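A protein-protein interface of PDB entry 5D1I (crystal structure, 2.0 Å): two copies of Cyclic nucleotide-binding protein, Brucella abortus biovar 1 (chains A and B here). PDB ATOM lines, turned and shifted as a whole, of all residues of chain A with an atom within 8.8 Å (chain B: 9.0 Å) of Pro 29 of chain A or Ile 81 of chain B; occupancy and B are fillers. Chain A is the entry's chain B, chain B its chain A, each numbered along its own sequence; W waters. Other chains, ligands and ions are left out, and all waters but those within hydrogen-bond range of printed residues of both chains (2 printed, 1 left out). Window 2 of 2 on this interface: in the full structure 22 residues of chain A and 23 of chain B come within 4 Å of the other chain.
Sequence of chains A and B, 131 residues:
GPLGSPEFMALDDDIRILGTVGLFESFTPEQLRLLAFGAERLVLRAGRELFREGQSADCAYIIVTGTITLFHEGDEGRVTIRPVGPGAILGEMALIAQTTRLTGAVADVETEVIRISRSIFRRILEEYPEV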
ATOM      1  N   ILE A  15     -25.766 -12.760  22.027  1.00  0.00           N
ATOM      2  CA  ILE A  15     -24.996 -13.835  21.408  1.00  0.00           C
ATOM      3  C   ILE A  15     -23.855 -14.264  22.319  1.00  0.00           C
ATOM      4  O   ILE A  15     -23.606 -15.456  22.511  1.00  0.00           O
ATOM      5  CB  ILE A  15     -24.411 -13.404  20.043  1.00  0.00           C
ATOM      6  CG1 ILE A  15     -25.528 -13.124  19.034  1.00  0.00           C
ATOM      7  CG2 ILE A  15     -23.454 -14.465  19.508  1.00  0.00           C
ATOM      8  CD1 ILE A  15     -26.010 -14.351  18.312  1.00  0.00           C
ATOM      9  N   LEU A  18     -25.247 -16.129  25.393  1.00  0.00           N
ATOM     10  CA  LEU A  18     -25.692 -17.463  24.995  1.00  0.00           C
ATOM     11  C   LEU A  18     -24.507 -18.412  24.824  1.00  0.00           C
ATOM     12  O   LEU A  18     -24.594 -19.597  25.147  1.00  0.00           O
ATOM     13  CB  LEU A  18     -26.507 -17.395  23.699  1.00  0.00           C
ATOM     14  CG  LEU A  18     -27.911 -16.790  23.816  1.00  0.00           C
ATOM     15  CD1 LEU A  18     -28.473 -16.472  22.440  1.00  0.00           C
ATOM     16  CD2 LEU A  18     -28.836 -17.732  24.557  1.00  0.00           C
ATOM     17  N   GLY A  19     -23.396 -17.877  24.335  1.00  0.00           N
ATOM     18  CA  GLY A  19     -22.198 -18.668  24.117  1.00  0.00           C
ATOM     19  C   GLY A  19     -21.500 -19.127  25.391  1.00  0.00           C
ATOM     20  O   GLY A  19     -20.585 -19.946  25.327  1.00  0.00           O
ATOM     21  N   PHE A  24     -24.724 -25.003  25.114  1.00  0.00           N
ATOM     22  CA  PHE A  24     -24.506 -24.315  23.837  1.00  0.00           C
ATOM     23  C   PHE A  24     -23.014 -24.202  23.536  1.00  0.00           C
ATOM     24  O   PHE A  24     -22.615 -23.490  22.614  1.00  0.00           O
ATOM     25  CB  PHE A  24     -25.122 -22.908  23.840  1.00  0.00           C
ATOM     26  CG  PHE A  24     -26.545 -22.846  24.344  1.00  0.00           C
ATOM     27  CD1 PHE A  24     -27.384 -23.944  24.272  1.00  0.00           C
ATOM     28  CD2 PHE A  24     -27.042 -21.671  24.882  1.00  0.00           C
ATOM     29  CE1 PHE A  24     -28.681 -23.876  24.743  1.00  0.00           C
ATOM     30  CE2 PHE A  24     -28.338 -21.595  25.352  1.00  0.00           C
ATOM     31  CZ  PHE A  24     -29.161 -22.698  25.279  1.00  0.00           C
ATOM     32  N   GLU A  25     -22.207 -24.903  24.328  1.00  0.00           N
ATOM     33  CA  GLU A  25     -20.744 -24.849  24.249  1.00  0.00           C
ATOM     34  C   GLU A  25     -20.192 -24.989  22.836  1.00  0.00           C
ATOM     35  O   GLU A  25     -19.333 -24.209  22.419  1.00  0.00           O
ATOM     36  CB  GLU A  25     -20.138 -25.949  25.132  1.00  0.00           C
ATOM     37  CG  GLU A  25     -18.628 -26.113  25.004  1.00  0.00           C
ATOM     38  CD  GLU A  25     -18.126 -27.392  25.655  1.00  0.00           C
ATOM     39  OE1 GLU A  25     -18.606 -27.733  26.756  1.00  0.00           O
ATOM     40  OE2 GLU A  25     -17.258 -28.064  25.061  1.00  0.00           O
ATOM     41  N   SER A  26     -20.684 -25.985  22.108  1.00  0.00           N
ATOM     42  CA  SER A  26     -20.143 -26.317  20.797  1.00  0.00           C
ATOM     43  C   SER A  26     -20.932 -25.693  19.651  1.00  0.00           C
ATOM     44  O   SER A  26     -20.707 -26.031  18.491  1.00  0.00           O
ATOM     45  CB  SER A  26     -20.108 -27.833  20.612  1.00  0.00           C
ATOM     46  OG  SER A  26     -21.426 -28.363  20.552  1.00  0.00           O
ATOM     47  N   PHE A  27     -21.862 -24.797  19.972  1.00  0.00           N
ATOM     48  CA  PHE A  27     -22.673 -24.168  18.934  1.00  0.00           C
ATOM     49  C   PHE A  27     -21.832 -23.276  18.031  1.00  0.00           C
ATOM     50  O   PHE A  27     -20.893 -22.615  18.474  1.00  0.00           O
ATOM     51  CB  PHE A  27     -23.817 -23.348  19.540  1.00  0.00           C
ATOM     52  CG  PHE A  27     -25.023 -24.168  19.926  1.00  0.00           C
ATOM     53  CD1 PHE A  27     -24.961 -25.549  19.958  1.00  0.00           C
ATOM     54  CD2 PHE A  27     -26.220 -23.550  20.245  1.00  0.00           C
ATOM     55  CE1 PHE A  27     -26.068 -26.299  20.315  1.00  0.00           C
ATOM     56  CE2 PHE A  27     -27.334 -24.295  20.598  1.00  0.00           C
ATOM     57  CZ  PHE A  27     -27.255 -25.670  20.633  1.00  0.00           C
ATOM     58  N   THR A  28     -22.184 -23.272  16.755  1.00  0.00           N
ATOM     59  CA  THR A  28     -21.584 -22.373  15.786  1.00  0.00           C
ATOM     60  C   THR A  28     -22.171 -20.981  15.984  1.00  0.00           C
ATOM     61  O   THR A  28     -23.216 -20.841  16.625  1.00  0.00           O
ATOM     62  CB  THR A  28     -21.850 -22.851  14.353  1.00  0.00           C
ATOM     63  OG1 THR A  28     -23.256 -22.779  14.089  1.00  0.00           O
ATOM     64  CG2 THR A  28     -21.379 -24.289  14.180  1.00  0.00           C
ATOM     65  N   PRO A  29     -21.504 -19.946  15.449  1.00  0.00           N
ATOM     66  CA  PRO A  29     -22.103 -18.607  15.500  1.00  0.00           C
ATOM     67  C   PRO A  29     -23.510 -18.573  14.909  1.00  0.00           C
ATOM     68  O   PRO A  29     -24.359 -17.825  15.394  1.00  0.00           O
ATOM     69  CB  PRO A  29     -21.136 -17.764  14.665  1.00  0.00           C
ATOM     70  CG  PRO A  29     -19.824 -18.432  14.846  1.00  0.00           C
ATOM     71  CD  PRO A  29     -20.125 -19.909  14.927  1.00  0.00           C
ATOM     72  N   GLU A  30     -23.755 -19.389  13.889  1.00  0.00           N
ATOM     73  CA  GLU A  30     -25.059 -19.432  13.247  1.00  0.00           C
ATOM     74  C   GLU A  30     -26.104 -20.015  14.183  1.00  0.00           C
ATOM     75  O   GLU A  30     -27.211 -19.492  14.281  1.00  0.00           O
ATOM     76  CB  GLU A  30     -25.005 -20.239  11.950  1.00  0.00           C
ATOM     77  CG  GLU A  30     -23.905 -19.802  10.993  1.00  0.00           C
ATOM     78  CD  GLU A  30     -22.663 -20.665  11.099  1.00  0.00           C
ATOM     79  OE1 GLU A  30     -21.693 -20.240  11.762  1.00  0.00           O
ATOM     80  OE2 GLU A  30     -22.658 -21.771  10.517  1.00  0.00           O
ATOM     81  N   GLN A  31     -25.750 -21.098  14.872  1.00  0.00           N
ATOM     82  CA  GLN A  31     -26.657 -21.709  15.839  1.00  0.00           C
ATOM     83  C   GLN A  31     -26.994 -20.741  16.969  1.00  0.00           C
ATOM     84  O   GLN A  31     -28.136 -20.683  17.427  1.00  0.00           O
ATOM     85  CB  GLN A  31     -26.058 -22.998  16.410  1.00  0.00           C
ATOM     86  CG  GLN A  31     -26.139 -24.198  15.477  1.00  0.00           C
ATOM     87  CD  GLN A  31     -25.432 -25.422  16.036  1.00  0.00           C
ATOM     88  OE1 GLN A  31     -24.248 -25.372  16.360  1.00  0.00           O
ATOM     89  NE2 GLN A  31     -26.161 -26.522  16.157  1.00  0.00           N
ATOM     90  N   LEU A  32     -26.000 -19.981  17.418  1.00  0.00           N
ATOM     91  CA  LEU A  32     -26.221 -19.008  18.483  1.00  0.00           C
ATOM     92  C   LEU A  32     -27.162 -17.901  18.024  1.00  0.00           C
ATOM     93  O   LEU A  32     -27.987 -17.415  18.798  1.00  0.00           O
ATOM     94  CB  LEU A  32     -24.897 -18.411  18.961  1.00  0.00           C
ATOM     95  CG  LEU A  32     -23.985 -19.339  19.762  1.00  0.00           C
ATOM     96  CD1 LEU A  32     -22.707 -18.607  20.173  1.00  0.00           C
ATOM     97  CD2 LEU A  32     -24.717 -19.885  20.985  1.00  0.00           C
ATOM     98  N   ARG A  33     -27.043 -17.513  16.758  1.00  0.00           N
ATOM     99  CA  ARG A  33     -27.932 -16.509  16.180  1.00  0.00           C
ATOM    100  C   ARG A  33     -29.379 -17.006  16.144  1.00  0.00           C
ATOM    101  O   ARG A  33     -30.298 -16.299  16.564  1.00  0.00           O
ATOM    102  CB  ARG A  33     -27.465 -16.134  14.775  1.00  0.00           C
ATOM    103  CG  ARG A  33     -27.275 -14.641  14.560  1.00  0.00           C
ATOM    104  CD  ARG A  33     -26.158 -14.379  13.564  1.00  0.00           C
ATOM    105  NE  ARG A  33     -26.230 -15.286  12.422  1.00  0.00           N
ATOM    106  CZ  ARG A  33     -25.170 -15.830  11.831  1.00  0.00           C
ATOM    107  NH1 ARG A  33     -25.332 -16.647  10.798  1.00  0.00           N
ATOM    108  NH2 ARG A  33     -23.948 -15.560  12.273  1.00  0.00           N
ATOM    109  N   LEU A  34     -29.570 -18.227  15.647  1.00  0.00           N
ATOM    110  CA  LEU A  34     -30.889 -18.854  15.620  1.00  0.00           C
ATOM    111  C   LEU A  34     -31.506 -18.862  17.004  1.00  0.00           C
ATOM    112  O   LEU A  34     -32.700 -18.612  17.176  1.00  0.00           O
ATOM    113  CB  LEU A  34     -30.799 -20.285  15.105  1.00  0.00           C
ATOM    114  CG  LEU A  34     -30.599 -20.553  13.625  1.00  0.00           C
ATOM    115  CD1 LEU A  34     -30.469 -22.052  13.429  1.00  0.00           C
ATOM    116  CD2 LEU A  34     -31.771 -20.001  12.826  1.00  0.00           C
ATOM    117  N   LEU A  35     -30.671 -19.165  17.986  1.00  0.00           N
ATOM    118  CA  LEU A  35     -31.068 -19.167  19.378  1.00  0.00           C
ATOM    119  C   LEU A  35     -31.538 -17.783  19.807  1.00  0.00           C
ATOM    120  O   LEU A  35     -32.609 -17.637  20.388  1.00  0.00           O
ATOM    121  CB  LEU A  35     -29.894 -19.625  20.243  1.00  0.00           C
ATOM    122  CG  LEU A  35     -30.134 -20.375  21.543  1.00  0.00           C
ATOM    123  CD1 LEU A  35     -31.197 -21.436  21.372  1.00  0.00           C
ATOM    124  CD2 LEU A  35     -28.820 -21.004  21.958  1.00  0.00           C
ATOM    125  N   ALA A  36     -30.728 -16.769  19.514  1.00  0.00           N
ATOM    126  CA  ALA A  36     -31.048 -15.400  19.892  1.00  0.00           C
ATOM    127  C   ALA A  36     -32.330 -14.918  19.213  1.00  0.00           C
ATOM    128  O   ALA A  36     -33.099 -14.149  19.790  1.00  0.00           O
ATOM    129  CB  ALA A  36     -29.891 -14.477  19.551  1.00  0.00           C
ATOM    130  N   PHE A  37     -32.551 -15.381  17.987  1.00  0.00           N
ATOM    131  CA  PHE A  37     -33.744 -15.021  17.226  1.00  0.00           C
ATOM    132  C   PHE A  37     -34.966 -15.830  17.653  1.00  0.00           C
ATOM    133  O   PHE A  37     -36.055 -15.281  17.828  1.00  0.00           O
ATOM    134  CB  PHE A  37     -33.496 -15.214  15.728  1.00  0.00           C
ATOM    135  CG  PHE A  37     -32.834 -14.042  15.068  1.00  0.00           C
ATOM    136  CD1 PHE A  37     -31.507 -13.738  15.328  1.00  0.00           C
ATOM    137  CD2 PHE A  37     -33.539 -13.243  14.182  1.00  0.00           C
ATOM    138  CE1 PHE A  37     -30.894 -12.655  14.717  1.00  0.00           C
ATOM    139  CE2 PHE A  37     -32.935 -12.160  13.571  1.00  0.00           C
ATOM    140  CZ  PHE A  37     -31.610 -11.865  13.837  1.00  0.00           C
ATOM    141  N   ILE A 124     -32.553 -26.176  17.118  1.00  0.00           N
ATOM    142  CA  ILE A 124     -31.230 -25.625  16.819  1.00  0.00           C
ATOM    143  C   ILE A 124     -30.213 -26.733  16.536  1.00  0.00           C
ATOM    144  O   ILE A 124     -29.308 -26.564  15.716  1.00  0.00           O
ATOM    145  CB  ILE A 124     -30.692 -24.748  17.981  1.00  0.00           C
ATOM    146  CG1 ILE A 124     -31.679 -23.643  18.348  1.00  0.00           C
ATOM    147  CG2 ILE A 124     -29.353 -24.131  17.626  1.00  0.00           C
ATOM    148  CD1 ILE A 124     -32.061 -22.767  17.208  1.00  0.00           C
ATOM    149  N   GLU B  53      -9.768 -32.131  21.029  1.00  0.00           N
ATOM    150  CA  GLU B  53     -11.086 -32.560  20.585  1.00  0.00           C
ATOM    151  C   GLU B  53     -11.200 -34.084  20.623  1.00  0.00           C
ATOM    152  O   GLU B  53     -10.325 -34.789  20.125  1.00  0.00           O
ATOM    153  CB  GLU B  53     -11.343 -32.041  19.172  1.00  0.00           C
ATOM    154  CG  GLU B  53     -12.718 -32.325  18.614  1.00  0.00           C
ATOM    155  CD  GLU B  53     -12.922 -31.666  17.264  1.00  0.00           C
ATOM    156  OE1 GLU B  53     -13.944 -30.973  17.082  1.00  0.00           O
ATOM    157  OE2 GLU B  53     -12.052 -31.833  16.386  1.00  0.00           O
ATOM    158  N   ILE B  68     -10.383 -17.604  24.649  1.00  0.00           N
ATOM    159  CA  ILE B  68     -10.105 -18.935  24.147  1.00  0.00           C
ATOM    160  C   ILE B  68     -10.847 -19.146  22.834  1.00  0.00           C
ATOM    161  O   ILE B  68     -12.044 -18.879  22.744  1.00  0.00           O
ATOM    162  CB  ILE B  68     -10.523 -20.014  25.167  1.00  0.00           C
ATOM    163  CG1 ILE B  68      -9.516 -20.077  26.317  1.00  0.00           C
ATOM    164  CG2 ILE B  68     -10.661 -21.376  24.500  1.00  0.00           C
ATOM    165  CD1 ILE B  68      -9.951 -20.981  27.454  1.00  0.00           C
ATOM    166  N   THR B  69     -10.132 -19.600  21.812  1.00  0.00           N
ATOM    167  CA  THR B  69     -10.766 -19.953  20.550  1.00  0.00           C
ATOM    168  C   THR B  69     -11.162 -21.425  20.536  1.00  0.00           C
ATOM    169  O   THR B  69     -10.332 -22.303  20.788  1.00  0.00           O
ATOM    170  CB  THR B  69      -9.844 -19.657  19.358  1.00  0.00           C
ATOM    171  OG1 THR B  69      -9.687 -18.244  19.227  1.00  0.00           O
ATOM    172  CG2 THR B  69     -10.433 -20.209  18.072  1.00  0.00           C
ATOM    173  N   LEU B  70     -12.438 -21.685  20.263  1.00  0.00           N
ATOM    174  CA  LEU B  70     -12.935 -23.043  20.089  1.00  0.00           C
ATOM    175  C   LEU B  70     -12.832 -23.425  18.624  1.00  0.00           C
ATOM    176  O   LEU B  70     -13.149 -22.622  17.750  1.00  0.00           O
ATOM    177  CB  LEU B  70     -14.384 -23.162  20.561  1.00  0.00           C
ATOM    178  CG  LEU B  70     -14.705 -22.686  21.976  1.00  0.00           C
ATOM    179  CD1 LEU B  70     -16.172 -22.942  22.292  1.00  0.00           C
ATOM    180  CD2 LEU B  70     -13.809 -23.379  22.992  1.00  0.00           C
ATOM    181  N   PHE B  71     -12.398 -24.648  18.344  1.00  0.00           N
ATOM    182  CA  PHE B  71     -12.193 -25.052  16.960  1.00  0.00           C
ATOM    183  C   PHE B  71     -12.464 -26.534  16.733  1.00  0.00           C
ATOM    184  O   PHE B  71     -12.522 -27.319  17.678  1.00  0.00           O
ATOM    185  CB  PHE B  71     -10.763 -24.708  16.514  1.00  0.00           C
ATOM    186  CG  PHE B  71      -9.684 -25.349  17.354  1.00  0.00           C
ATOM    187  CD1 PHE B  71      -9.222 -26.625  17.064  1.00  0.00           C
ATOM    188  CD2 PHE B  71      -9.121 -24.669  18.420  1.00  0.00           C
ATOM    189  CE1 PHE B  71      -8.226 -27.211  17.830  1.00  0.00           C
ATOM    190  CE2 PHE B  71      -8.129 -25.249  19.189  1.00  0.00           C
ATOM    191  CZ  PHE B  71      -7.679 -26.519  18.894  1.00  0.00           C
ATOM    192  N   HIS B  72     -12.640 -26.903  15.468  1.00  0.00           N
ATOM    193  CA  HIS B  72     -12.745 -28.303  15.081  1.00  0.00           C
ATOM    194  C   HIS B  72     -11.495 -28.716  14.323  1.00  0.00           C
ATOM    195  O   HIS B  72     -10.964 -27.937  13.537  1.00  0.00           O
ATOM    196  CB  HIS B  72     -13.988 -28.548  14.221  1.00  0.00           C
ATOM    197  CG  HIS B  72     -15.265 -28.590  15.001  1.00  0.00           C
ATOM    198  ND1 HIS B  72     -15.453 -29.438  16.071  1.00  0.00           N
ATOM    199  CD2 HIS B  72     -16.418 -27.894  14.865  1.00  0.00           C
ATOM    200  CE1 HIS B  72     -16.666 -29.260  16.564  1.00  0.00           C
ATOM    201  NE2 HIS B  72     -17.273 -28.327  15.851  1.00  0.00           N
ATOM    202  N   GLU B  73     -11.026 -29.934  14.563  1.00  0.00           N
ATOM    203  CA  GLU B  73      -9.866 -30.446  13.845  1.00  0.00           C
ATOM    204  C   GLU B  73     -10.293 -30.941  12.464  1.00  0.00           C
ATOM    205  O   GLU B  73     -10.956 -31.972  12.344  1.00  0.00           O
ATOM    206  CB  GLU B  73      -9.192 -31.567  14.639  1.00  0.00           C
ATOM    207  CG  GLU B  73      -7.671 -31.551  14.570  1.00  0.00           C
ATOM    208  CD  GLU B  73      -7.043 -30.575  15.550  1.00  0.00           C
ATOM    209  OE1 GLU B  73      -7.415 -30.597  16.744  1.00  0.00           O
ATOM    210  OE2 GLU B  73      -6.173 -29.788  15.122  1.00  0.00           O
ATOM    211  N   ARG B  78      -6.812 -27.013  11.911  1.00  0.00           N
ATOM    212  CA  ARG B  78      -7.868 -26.422  12.724  1.00  0.00           C
ATOM    213  C   ARG B  78      -8.862 -25.611  11.899  1.00  0.00           C
ATOM    214  O   ARG B  78      -8.485 -24.928  10.949  1.00  0.00           O
ATOM    215  CB  ARG B  78      -7.272 -25.513  13.795  1.00  0.00           C
ATOM    216  CG  ARG B  78      -6.469 -26.205  14.871  1.00  0.00           C
ATOM    217  CD  ARG B  78      -5.973 -25.156  15.841  1.00  0.00           C
ATOM    218  NE  ARG B  78      -5.153 -25.695  16.917  1.00  0.00           N
ATOM    219  CZ  ARG B  78      -4.384 -24.941  17.693  1.00  0.00           C
ATOM    220  NH1 ARG B  78      -4.329 -23.630  17.492  1.00  0.00           N
ATOM    221  NH2 ARG B  78      -3.659 -25.491  18.657  1.00  0.00           N
ATOM    222  N   VAL B  79     -10.133 -25.688  12.278  1.00  0.00           N
ATOM    223  CA  VAL B  79     -11.151 -24.805  11.727  1.00  0.00           C
ATOM    224  C   VAL B  79     -11.880 -24.121  12.880  1.00  0.00           C
ATOM    225  O   VAL B  79     -12.544 -24.771  13.690  1.00  0.00           O
ATOM    226  CB  VAL B  79     -12.155 -25.559  10.830  1.00  0.00           C
ATOM    227  CG1 VAL B  79     -13.241 -24.613  10.340  1.00  0.00           C
ATOM    228  CG2 VAL B  79     -11.435 -26.203   9.651  1.00  0.00           C
ATOM    229  N   THR B  80     -11.732 -22.804  12.953  1.00  0.00           N
ATOM    230  CA  THR B  80     -12.260 -22.019  14.059  1.00  0.00           C
ATOM    231  C   THR B  80     -13.784 -22.073  14.132  1.00  0.00           C
ATOM    232  O   THR B  80     -14.470 -21.987  13.114  1.00  0.00           O
ATOM    233  CB  THR B  80     -11.797 -20.546  13.942  1.00  0.00           C
ATOM    234  OG1 THR B  80     -10.381 -20.479  14.157  1.00  0.00           O
ATOM    235  CG2 THR B  80     -12.497 -19.662  14.960  1.00  0.00           C
ATOM    236  N   ILE B  81     -14.307 -22.242  15.343  1.00  0.00           N
ATOM    237  CA  ILE B  81     -15.740 -22.133  15.581  1.00  0.00           C
ATOM    238  C   ILE B  81     -16.087 -20.708  15.990  1.00  0.00           C
ATOM    239  O   ILE B  81     -16.740 -19.978  15.245  1.00  0.00           O
ATOM    240  CB  ILE B  81     -16.214 -23.101  16.677  1.00  0.00           C
ATOM    241  CG1 ILE B  81     -15.848 -24.538  16.310  1.00  0.00           C
ATOM    242  CG2 ILE B  81     -17.711 -22.976  16.882  1.00  0.00           C
ATOM    243  CD1 ILE B  81     -16.217 -25.537  17.372  1.00  0.00           C
ATOM    244  N   ARG B  82     -15.625 -20.322  17.176  1.00  0.00           N
ATOM    245  CA  ARG B  82     -15.886 -19.000  17.736  1.00  0.00           C
ATOM    246  C   ARG B  82     -14.995 -18.787  18.957  1.00  0.00           C
ATOM    247  O   ARG B  82     -14.486 -19.752  19.523  1.00  0.00           O
ATOM    248  CB  ARG B  82     -17.360 -18.861  18.129  1.00  0.00           C
ATOM    249  CG  ARG B  82     -17.735 -19.718  19.330  1.00  0.00           C
ATOM    250  CD  ARG B  82     -19.194 -19.569  19.728  1.00  0.00           C
ATOM    251  NE  ARG B  82     -19.368 -19.861  21.148  1.00  0.00           N
ATOM    252  CZ  ARG B  82     -19.560 -21.079  21.638  1.00  0.00           C
ATOM    253  NH1 ARG B  82     -19.614 -22.119  20.821  1.00  0.00           N
ATOM    254  NH2 ARG B  82     -19.693 -21.255  22.944  1.00  0.00           N
ATOM    255  N   PRO B  83     -14.795 -17.526  19.366  1.00  0.00           N
ATOM    256  CA  PRO B  83     -14.065 -17.270  20.615  1.00  0.00           C
ATOM    257  C   PRO B  83     -14.978 -17.279  21.843  1.00  0.00           C
ATOM    258  O   PRO B  83     -16.163 -16.974  21.726  1.00  0.00           O
ATOM    259  CB  PRO B  83     -13.475 -15.878  20.389  1.00  0.00           C
ATOM    260  CG  PRO B  83     -14.460 -15.212  19.491  1.00  0.00           C
ATOM    261  CD  PRO B  83     -14.992 -16.294  18.580  1.00  0.00           C
ATOM    262  N   VAL B  84     -14.435 -17.638  23.004  1.00  0.00           N
ATOM    263  CA  VAL B  84     -15.178 -17.529  24.260  1.00  0.00           C
ATOM    264  C   VAL B  84     -14.376 -16.736  25.285  1.00  0.00           C
ATOM    265  O   VAL B  84     -13.142 -16.748  25.267  1.00  0.00           O
ATOM    266  CB  VAL B  84     -15.539 -18.911  24.846  1.00  0.00           C
ATOM    267  CG1 VAL B  84     -16.691 -19.531  24.067  1.00  0.00           C
ATOM    268  CG2 VAL B  84     -14.319 -19.834  24.860  1.00  0.00           C
ATOM    269  N   LEU B 102     -16.045 -31.808  23.012  1.00  0.00           N
ATOM    270  CA  LEU B 102     -16.769 -31.570  21.767  1.00  0.00           C
ATOM    271  C   LEU B 102     -15.961 -30.768  20.753  1.00  0.00           C
ATOM    272  O   LEU B 102     -16.164 -30.891  19.544  1.00  0.00           O
ATOM    273  CB  LEU B 102     -18.086 -30.851  22.050  1.00  0.00           C
ATOM    274  CG  LEU B 102     -19.152 -31.669  22.780  1.00  0.00           C
ATOM    275  CD1 LEU B 102     -20.393 -30.821  23.029  1.00  0.00           C
ATOM    276  CD2 LEU B 102     -19.503 -32.916  21.985  1.00  0.00           C
ATOM    277  N   THR B 103     -15.061 -29.926  21.246  1.00  0.00           N
ATOM    278  CA  THR B 103     -14.225 -29.106  20.373  1.00  0.00           C
ATOM    279  C   THR B 103     -12.788 -29.085  20.863  1.00  0.00           C
ATOM    280  O   THR B 103     -12.485 -29.574  21.950  1.00  0.00           O
ATOM    281  CB  THR B 103     -14.711 -27.648  20.312  1.00  0.00           C
ATOM    282  OG1 THR B 103     -14.253 -26.959  21.482  1.00  0.00           O
ATOM    283  CG2 THR B 103     -16.235 -27.572  20.249  1.00  0.00           C
ATOM    284  N   GLY B 104     -11.905 -28.505  20.061  1.00  0.00           N
ATOM    285  CA  GLY B 104     -10.589 -28.137  20.546  1.00  0.00           C
ATOM    286  C   GLY B 104     -10.722 -26.786  21.221  1.00  0.00           C
ATOM    287  O   GLY B 104     -11.744 -26.115  21.073  1.00  0.00           O
ATOM    288  N   ALA B 105      -9.705 -26.390  21.975  1.00  0.00           N
ATOM    289  CA  ALA B 105      -9.698 -25.092  22.641  1.00  0.00           C
ATOM    290  C   ALA B 105      -8.270 -24.625  22.861  1.00  0.00           C
ATOM    291  O   ALA B 105      -7.452 -25.363  23.401  1.00  0.00           O
ATOM    292  CB  ALA B 105     -10.436 -25.167  23.963  1.00  0.00           C
HETATM  293  O   HOH W   1     -14.784 -28.841  24.312  1.00  0.00           O
HETATM  294  O   HOH W   2     -19.545 -27.523  16.629  1.00  0.00           O
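The backbone carbonyl oxygen (O) of Gly 19 of chain A is in hydrogen-bond range of the guanidinium group (NH2) of Arg 82 of chain B, at 2.9 Å.
The guanidinium group of Arg 82 of chain B sits at hydrogen-bond distance from the backbone carbonyl oxygen of Glu 25 of chain A.
The guanidinium group (NH1) of Arg 82 of chain B lies within hydrogen-bond range of the backbone carbonyl oxygen (O) of Phe 27 of chain A (2.7 Å).
N of Ile 81 of chain B is in hydrogen-bond range of O of Leu 70 of chain B (2.7 Å).
O of Arg 82 of chain B is in hydrogen-bond range of N of Leu 70 of chain B (2.9 Å).
Among the printed residues, pairs that only touch across the chains: Pro 29 of chain A with Ile 81 of chain B (3.4 Å), Glu 25 of chain A with Leu 70 of chain B (3.4 Å), Phe 27 of chain A with Ile 81 of chain B (3.6 Å), Ser 26 of chain A with Leu 102 of chain B (3.6 Å), Leu 32 of chain A with Arg 82 of chain B (3.7 Å), Phe 24 of chain A with Arg 82 of chain B (3.7 Å), Ser 26 of chain A with Thr 103 of chain B (3.9 Å) and Ser 26 of chain A with Arg 82 of chain B (3.98 Å).
Of the printed residues of chain B, Gly 19 of chain A touches Arg 82 (2.9 Å).
Of the printed residues of chain B, Phe 24 of chain A touches Arg 82.
Of the printed residues of chain B, Glu 25 of chain A touches Leu 70 and Arg 82.
Printed residues of chain B within 4 Å of Pro 29 of chain A: Ile 81.
Arg 33 of chain A touches none of the printed residues of chain B.
Glu 73 of chain B touches none of the printed residues of chain A.
No residue of chain A comes within 4 Å of Thr 80 of chain B.
Printed residues of chain A within 4 Å of Arg 82 of chain B: Gly 19, Phe 24, Glu 25, Ser 26, Phe 27 and Leu 32.
Of the 18 printed residues of chain B, 5 touch a printed residue of chain A.
Hydrophobic or aromatic side chains of chain A that line the printed part of chain B: Pro 29 and Leu 32.
Along chain A the printed residues that touch a printed residue of chain B span positions 19 to 32.
Among the printed residues, 11 pairs touch across the chains.
Among the printed residues, no Asp or Glu carboxylate lies within 4 Å of a Lys or Arg side-chain nitrogen of the other chain.
No position is printed for both chains.
Water W2 lies within hydrogen-bond range of a ring nitrogen (NE2) of His 72 of chain B (2.5 Å) and the backbone carbonyl oxygen of Ser 26 of chain A (2.7 Å).
Water W1 lies within hydrogen-bond range of the side-chain carboxylate of Glu 25 of chain A (2.7 Å), the backbone NH of Thr 103 of chain B (3.3 Å) and the backbone NH of Leu 102 of chain B (3.5 Å).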
